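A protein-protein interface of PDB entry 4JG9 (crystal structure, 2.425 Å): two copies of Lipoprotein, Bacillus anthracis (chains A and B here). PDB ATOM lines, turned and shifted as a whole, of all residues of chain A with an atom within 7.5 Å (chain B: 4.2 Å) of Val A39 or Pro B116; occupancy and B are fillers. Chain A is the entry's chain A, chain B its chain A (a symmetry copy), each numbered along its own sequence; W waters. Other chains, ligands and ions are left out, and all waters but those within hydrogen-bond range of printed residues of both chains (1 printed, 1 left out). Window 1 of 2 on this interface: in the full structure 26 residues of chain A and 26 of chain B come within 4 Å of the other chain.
The backbone NH (N) of Asn A40 is in hydrogen-bond range of the side-chain hydroxyl (OG1) of Thr B117 (2.8 Å).
The side-chain hydroxyl of Ser A36 is in hydrogen-bond range of the backbone NH of Gln A38. The backbone carbonyl oxygen (O) of Ala B108 lies within hydrogen-bond range of the backbone NH (N) of Thr B117 (2.9 Å). The side-chain hydroxyl (OG1) of Thr A37 sits at hydrogen-bond distance from the side-chain amide nitrogen (NE2) of Gln A38, 2.8 Å away.
Pro B150 touches Ser A36 (CB to O, 3.5 Å). Pro B150 touches Thr A37. Thr B117 touches Gln A38. Pro B150 touches Gln A38 (CG to C, 3.9 Å). Pro B116 touches Val A39. Val A39 touches Thr B117 (CA to OG1, 3.4 Å). Asn A40 touches Pro B150. Thr A115 touches Val B39 (CG2 to CG1, 3.5 Å). Thr A115 touches Thr B115. Thr A117 touches Val B39 (OG1 to CA, 3.4 Å).
Of the printed residues of chain B, Gln A38 touches Thr B117 and Pro B150. Of the printed residues of chain B, Val A39 touches Thr B115 (3.5 Å), Pro B116 (3.9 Å), Thr B117 (3.4 Å) and Pro B150 (3.5 Å). Printed residues of chain B within 4 Å of Asn A40: Thr B117 and Pro B150. Trp A130 touches none of the printed residues of chain B. Of the printed residues of chain A, Val B39 touches Thr A115, Pro A116 and Thr A117. Printed residues of chain A within 4 Å of Pro B116: Val A39.
Printed residues of chain A that touch a printed residue of chain B: Ser A36, Thr A37, Gln A38, Val A39, Asn A40, Thr A115, Pro A116 and Thr A117. Of the 11 printed residues of chain B, 5 touch a printed residue of chain A. Hydrophobic or aromatic side chains of chain B within 4 Å of the printed part of chain A: Val B39 and Pro B150. Along chain B the printed residues that touch a printed residue of chain A span positions 39 to 150. Among the printed residues, 14 pairs touch across the chains.
Val A39 touches Thr B115, and with the chains exchanged Thr A115 touches Val B39. Val A39 touches Pro B116, and with the chains exchanged Pro A116 touches Val B39. Val A39 touches Thr B117, and with the chains exchanged Thr A117 touches Val B39. Thr B115 touches its own counterpart, Thr A115. Of the 14 pairs that touch across the chains among the printed residues, 7 have their exchanged pair printed and touching as well.
Water W1 lies within hydrogen-bond range of the side-chain amide oxygen of Gln A38 (2.9 Å) and the side-chain hydroxyl of Thr B115 (3.2 Å).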
ATOM      1  N   SER A  36     -29.962  13.830  17.720  1.00  0.00           N
ATOM      2  CA  SER A  36     -28.905  14.831  17.587  1.00  0.00           C
ATOM      3  C   SER A  36     -28.607  15.127  16.113  1.00  0.00           C
ATOM      4  O   SER A  36     -28.652  14.245  15.256  1.00  0.00           O
ATOM      5  CB  SER A  36     -27.624  14.377  18.319  1.00  0.00           C
ATOM      6  OG  SER A  36     -26.563  15.321  18.180  1.00  0.00           O
ATOM      7  N   THR A  37     -28.299  16.382  15.835  1.00  0.00           N
ATOM      8  CA  THR A  37     -27.912  16.803  14.507  1.00  0.00           C
ATOM      9  C   THR A  37     -26.421  16.551  14.307  1.00  0.00           C
ATOM     10  O   THR A  37     -25.926  16.600  13.181  1.00  0.00           O
ATOM     11  CB  THR A  37     -28.158  18.311  14.312  1.00  0.00           C
ATOM     12  OG1 THR A  37     -27.530  19.031  15.380  1.00  0.00           O
ATOM     13  CG2 THR A  37     -29.641  18.632  14.303  1.00  0.00           C
ATOM     14  N   GLN A  38     -25.716  16.260  15.401  1.00  0.00           N
ATOM     15  CA  GLN A  38     -24.255  16.314  15.392  1.00  0.00           C
ATOM     16  C   GLN A  38     -23.523  14.976  15.356  1.00  0.00           C
ATOM     17  O   GLN A  38     -22.403  14.892  14.841  1.00  0.00           O
ATOM     18  CB  GLN A  38     -23.792  17.133  16.593  1.00  0.00           C
ATOM     19  CG  GLN A  38     -24.458  18.511  16.643  1.00  0.00           C
ATOM     20  CD  GLN A  38     -24.018  19.412  15.509  1.00  0.00           C
ATOM     21  OE1 GLN A  38     -22.826  19.543  15.240  1.00  0.00           O
ATOM     22  NE2 GLN A  38     -24.981  20.000  14.806  1.00  0.00           N
ATOM     23  N   VAL A  39     -24.125  13.941  15.929  1.00  0.00           N
ATOM     24  CA  VAL A  39     -23.483  12.627  15.976  1.00  0.00           C
ATOM     25  C   VAL A  39     -24.494  11.526  15.716  1.00  0.00           C
ATOM     26  O   VAL A  39     -25.703  11.738  15.864  1.00  0.00           O
ATOM     27  CB  VAL A  39     -22.820  12.339  17.342  1.00  0.00           C
ATOM     28  CG1 VAL A  39     -21.824  13.426  17.699  1.00  0.00           C
ATOM     29  CG2 VAL A  39     -23.882  12.205  18.420  1.00  0.00           C
ATOM     30  N   ASN A  40     -23.993  10.350  15.346  1.00  0.00           N
ATOM     31  CA  ASN A  40     -24.827   9.158  15.246  1.00  0.00           C
ATOM     32  C   ASN A  40     -24.903   8.439  16.593  1.00  0.00           C
ATOM     33  O   ASN A  40     -24.004   8.550  17.427  1.00  0.00           O
ATOM     34  CB  ASN A  40     -24.274   8.198  14.197  1.00  0.00           C
ATOM     35  CG  ASN A  40     -24.643   8.605  12.787  1.00  0.00           C
ATOM     36  OD1 ASN A  40     -25.783   9.007  12.535  1.00  0.00           O
ATOM     37  ND2 ASN A  40     -23.683   8.513  11.858  1.00  0.00           N
ATOM     38  N   ALA A  41     -25.969   7.677  16.780  1.00  0.00           N
ATOM     39  CA  ALA A  41     -26.151   6.891  17.983  1.00  0.00           C
ATOM     40  C   ALA A  41     -26.765   5.561  17.557  1.00  0.00           C
ATOM     41  O   ALA A  41     -27.264   5.437  16.441  1.00  0.00           O
ATOM     42  CB  ALA A  41     -27.063   7.622  18.954  1.00  0.00           C
ATOM     43  N   VAL A 114     -27.296  16.610  24.592  1.00  0.00           N
ATOM     44  CA  VAL A 114     -28.170  15.731  23.815  1.00  0.00           C
ATOM     45  C   VAL A 114     -27.299  14.851  22.924  1.00  0.00           C
ATOM     46  O   VAL A 114     -27.774  14.214  21.989  1.00  0.00           O
ATOM     47  CB  VAL A 114     -29.184  16.527  22.959  1.00  0.00           C
ATOM     48  CG1 VAL A 114     -30.159  17.274  23.850  1.00  0.00           C
ATOM     49  CG2 VAL A 114     -28.456  17.480  22.015  1.00  0.00           C
ATOM     50  N   THR A 115     -26.006  14.838  23.219  1.00  0.00           N
ATOM     51  CA  THR A 115     -25.036  14.128  22.396  1.00  0.00           C
ATOM     52  C   THR A 115     -24.544  12.864  23.104  1.00  0.00           C
ATOM     53  O   THR A 115     -23.702  12.935  23.991  1.00  0.00           O
ATOM     54  CB  THR A 115     -23.833  15.017  22.112  1.00  0.00           C
ATOM     55  OG1 THR A 115     -24.288  16.311  21.716  1.00  0.00           O
ATOM     56  CG2 THR A 115     -23.004  14.430  21.018  1.00  0.00           C
ATOM     57  N   PRO A 116     -25.060  11.697  22.699  1.00  0.00           N
ATOM     58  CA  PRO A 116     -24.672  10.446  23.355  1.00  0.00           C
ATOM     59  C   PRO A 116     -23.258  10.038  22.976  1.00  0.00           C
ATOM     60  O   PRO A 116     -22.752  10.430  21.928  1.00  0.00           O
ATOM     61  CB  PRO A 116     -25.674   9.432  22.803  1.00  0.00           C
ATOM     62  CG  PRO A 116     -26.057   9.990  21.459  1.00  0.00           C
ATOM     63  CD  PRO A 116     -26.057  11.488  21.633  1.00  0.00           C
ATOM     64  N   THR A 117     -22.602   9.305  23.854  1.00  0.00           N
ATOM     65  CA  THR A 117     -21.259   8.849  23.590  1.00  0.00           C
ATOM     66  C   THR A 117     -21.048   7.503  24.235  1.00  0.00           C
ATOM     67  O   THR A 117     -21.693   7.170  25.215  1.00  0.00           O
ATOM     68  CB  THR A 117     -20.213   9.845  24.116  1.00  0.00           C
ATOM     69  OG1 THR A 117     -18.912   9.461  23.670  1.00  0.00           O
ATOM     70  CG2 THR A 117     -20.228   9.887  25.618  1.00  0.00           C
ATOM     71  N   TRP A 130     -19.781   1.015  22.253  1.00  0.00           N
ATOM     72  CA  TRP A 130     -21.084   1.112  22.901  1.00  0.00           C
ATOM     73  C   TRP A 130     -21.347  -0.126  23.730  1.00  0.00           C
ATOM     74  O   TRP A 130     -21.995  -0.063  24.787  1.00  0.00           O
ATOM     75  CB  TRP A 130     -22.214   1.204  21.865  1.00  0.00           C
ATOM     76  CG  TRP A 130     -22.065   2.276  20.817  1.00  0.00           C
ATOM     77  CD1 TRP A 130     -21.620   2.114  19.534  1.00  0.00           C
ATOM     78  CD2 TRP A 130     -22.398   3.664  20.952  1.00  0.00           C
ATOM     79  NE1 TRP A 130     -21.654   3.321  18.863  1.00  0.00           N
ATOM     80  CE2 TRP A 130     -22.117   4.288  19.717  1.00  0.00           C
ATOM     81  CE3 TRP A 130     -22.909   4.441  22.000  1.00  0.00           C
ATOM     82  CZ2 TRP A 130     -22.325   5.655  19.497  1.00  0.00           C
ATOM     83  CZ3 TRP A 130     -23.106   5.807  21.781  1.00  0.00           C
ATOM     84  CH2 TRP A 130     -22.813   6.395  20.534  1.00  0.00           C
ATOM     85  N   VAL B  39     -17.997  14.085  24.087  1.00  0.00           N
ATOM     86  CA  VAL B  39     -18.000  12.703  23.607  1.00  0.00           C
ATOM     87  C   VAL B  39     -16.594  12.134  23.600  1.00  0.00           C
ATOM     88  O   VAL B  39     -15.613  12.887  23.607  1.00  0.00           O
ATOM     89  CB  VAL B  39     -18.564  12.573  22.175  1.00  0.00           C
ATOM     90  CG1 VAL B  39     -19.958  13.165  22.086  1.00  0.00           C
ATOM     91  CG2 VAL B  39     -17.629  13.243  21.182  1.00  0.00           C
ATOM     92  N   ALA B  41     -13.661   9.828  21.549  1.00  0.00           N
ATOM     93  CA  ALA B  41     -13.237   9.596  20.184  1.00  0.00           C
ATOM     94  C   ALA B  41     -12.076   8.610  20.238  1.00  0.00           C
ATOM     95  O   ALA B  41     -11.496   8.394  21.300  1.00  0.00           O
ATOM     96  CB  ALA B  41     -12.809  10.905  19.539  1.00  0.00           C
ATOM     97  N   PHE B  45      -7.477  10.015  16.881  1.00  0.00           N
ATOM     98  CA  PHE B  45      -8.105  11.189  16.317  1.00  0.00           C
ATOM     99  C   PHE B  45      -7.718  12.446  17.069  1.00  0.00           C
ATOM    100  O   PHE B  45      -7.824  12.511  18.283  1.00  0.00           O
ATOM    101  CB  PHE B  45      -9.622  11.077  16.317  1.00  0.00           C
ATOM    102  CG  PHE B  45     -10.308  12.370  16.009  1.00  0.00           C
ATOM    103  CD1 PHE B  45     -10.434  12.804  14.709  1.00  0.00           C
ATOM    104  CD2 PHE B  45     -10.796  13.167  17.020  1.00  0.00           C
ATOM    105  CE1 PHE B  45     -11.052  13.999  14.419  1.00  0.00           C
ATOM    106  CE2 PHE B  45     -11.413  14.364  16.739  1.00  0.00           C
ATOM    107  CZ  PHE B  45     -11.543  14.780  15.436  1.00  0.00           C
ATOM    108  N   ILE B 107     -13.819   8.940  10.473  1.00  0.00           N
ATOM    109  CA  ILE B 107     -14.289   9.783  11.560  1.00  0.00           C
ATOM    110  C   ILE B 107     -14.803  11.092  10.979  1.00  0.00           C
ATOM    111  O   ILE B 107     -14.032  11.850  10.391  1.00  0.00           O
ATOM    112  CB  ILE B 107     -13.149  10.098  12.525  1.00  0.00           C
ATOM    113  CG1 ILE B 107     -12.548   8.797  13.080  1.00  0.00           C
ATOM    114  CG2 ILE B 107     -13.628  11.018  13.636  1.00  0.00           C
ATOM    115  CD1 ILE B 107     -11.514   9.023  14.167  1.00  0.00           C
ATOM    116  N   ALA B 108     -16.089  11.371  11.172  1.00  0.00           N
ATOM    117  CA  ALA B 108     -16.740  12.515  10.535  1.00  0.00           C
ATOM    118  C   ALA B 108     -17.001  13.657  11.506  1.00  0.00           C
ATOM    119  O   ALA B 108     -17.252  13.441  12.709  1.00  0.00           O
ATOM    120  CB  ALA B 108     -18.043  12.080   9.889  1.00  0.00           C
ATOM    121  N   LEU B 109     -16.910  14.876  10.995  1.00  0.00           N
ATOM    122  CA  LEU B 109     -17.324  16.052  11.757  1.00  0.00           C
ATOM    123  C   LEU B 109     -18.102  16.996  10.871  1.00  0.00           C
ATOM    124  O   LEU B 109     -17.717  17.267   9.728  1.00  0.00           O
ATOM    125  CB  LEU B 109     -16.127  16.793  12.349  1.00  0.00           C
ATOM    126  CG  LEU B 109     -15.428  16.037  13.480  1.00  0.00           C
ATOM    127  CD1 LEU B 109     -14.133  15.415  12.984  1.00  0.00           C
ATOM    128  CD2 LEU B 109     -15.199  16.948  14.682  1.00  0.00           C
ATOM    129  N   VAL B 114     -16.932  20.307  16.848  1.00  0.00           N
ATOM    130  CA  VAL B 114     -15.709  19.713  17.389  1.00  0.00           C
ATOM    131  C   VAL B 114     -16.042  18.321  17.916  1.00  0.00           C
ATOM    132  O   VAL B 114     -15.271  17.710  18.652  1.00  0.00           O
ATOM    133  CB  VAL B 114     -15.089  20.578  18.511  1.00  0.00           C
ATOM    134  CG1 VAL B 114     -14.605  21.903  17.953  1.00  0.00           C
ATOM    135  CG2 VAL B 114     -16.092  20.790  19.642  1.00  0.00           C
ATOM    136  N   THR B 115     -17.216  17.830  17.540  1.00  0.00           N
ATOM    137  CA  THR B 115     -17.717  16.559  18.046  1.00  0.00           C
ATOM    138  C   THR B 115     -17.653  15.480  16.962  1.00  0.00           C
ATOM    139  O   THR B 115     -18.501  15.435  16.080  1.00  0.00           O
ATOM    140  CB  THR B 115     -19.164  16.702  18.496  1.00  0.00           C
ATOM    141  OG1 THR B 115     -19.294  17.883  19.288  1.00  0.00           O
ATOM    142  CG2 THR B 115     -19.573  15.516  19.305  1.00  0.00           C
ATOM    143  N   PRO B 116     -16.652  14.596  17.039  1.00  0.00           N
ATOM    144  CA  PRO B 116     -16.497  13.558  16.016  1.00  0.00           C
ATOM    145  C   PRO B 116     -17.560  12.481  16.157  1.00  0.00           C
ATOM    146  O   PRO B 116     -18.111  12.281  17.236  1.00  0.00           O
ATOM    147  CB  PRO B 116     -15.117  12.973  16.312  1.00  0.00           C
ATOM    148  CG  PRO B 116     -14.923  13.216  17.784  1.00  0.00           C
ATOM    149  CD  PRO B 116     -15.592  14.539  18.063  1.00  0.00           C
ATOM    150  N   THR B 117     -17.888  11.831  15.057  1.00  0.00           N
ATOM    151  CA  THR B 117     -18.873  10.778  15.079  1.00  0.00           C
ATOM    152  C   THR B 117     -18.518   9.734  14.051  1.00  0.00           C
ATOM    153  O   THR B 117     -17.863  10.024  13.064  1.00  0.00           O
ATOM    154  CB  THR B 117     -20.285  11.322  14.800  1.00  0.00           C
ATOM    155  OG1 THR B 117     -21.251  10.293  15.020  1.00  0.00           O
ATOM    156  CG2 THR B 117     -20.395  11.808  13.383  1.00  0.00           C
ATOM    157  N   PRO B 150     -26.181  12.243  10.454  1.00  0.00           N
ATOM    158  CA  PRO B 150     -27.322  12.641  11.286  1.00  0.00           C
ATOM    159  C   PRO B 150     -28.051  13.906  10.851  1.00  0.00           C
ATOM    160  O   PRO B 150     -29.214  14.057  11.215  1.00  0.00           O
ATOM    161  CB  PRO B 150     -26.697  12.854  12.673  1.00  0.00           C
ATOM    162  CG  PRO B 150     -25.249  13.088  12.418  1.00  0.00           C
ATOM    163  CD  PRO B 150     -24.904  12.297  11.187  1.00  0.00           C
HETATM  164  O   HOH W   1     -21.784  19.339  17.917  1.00  0.00           O
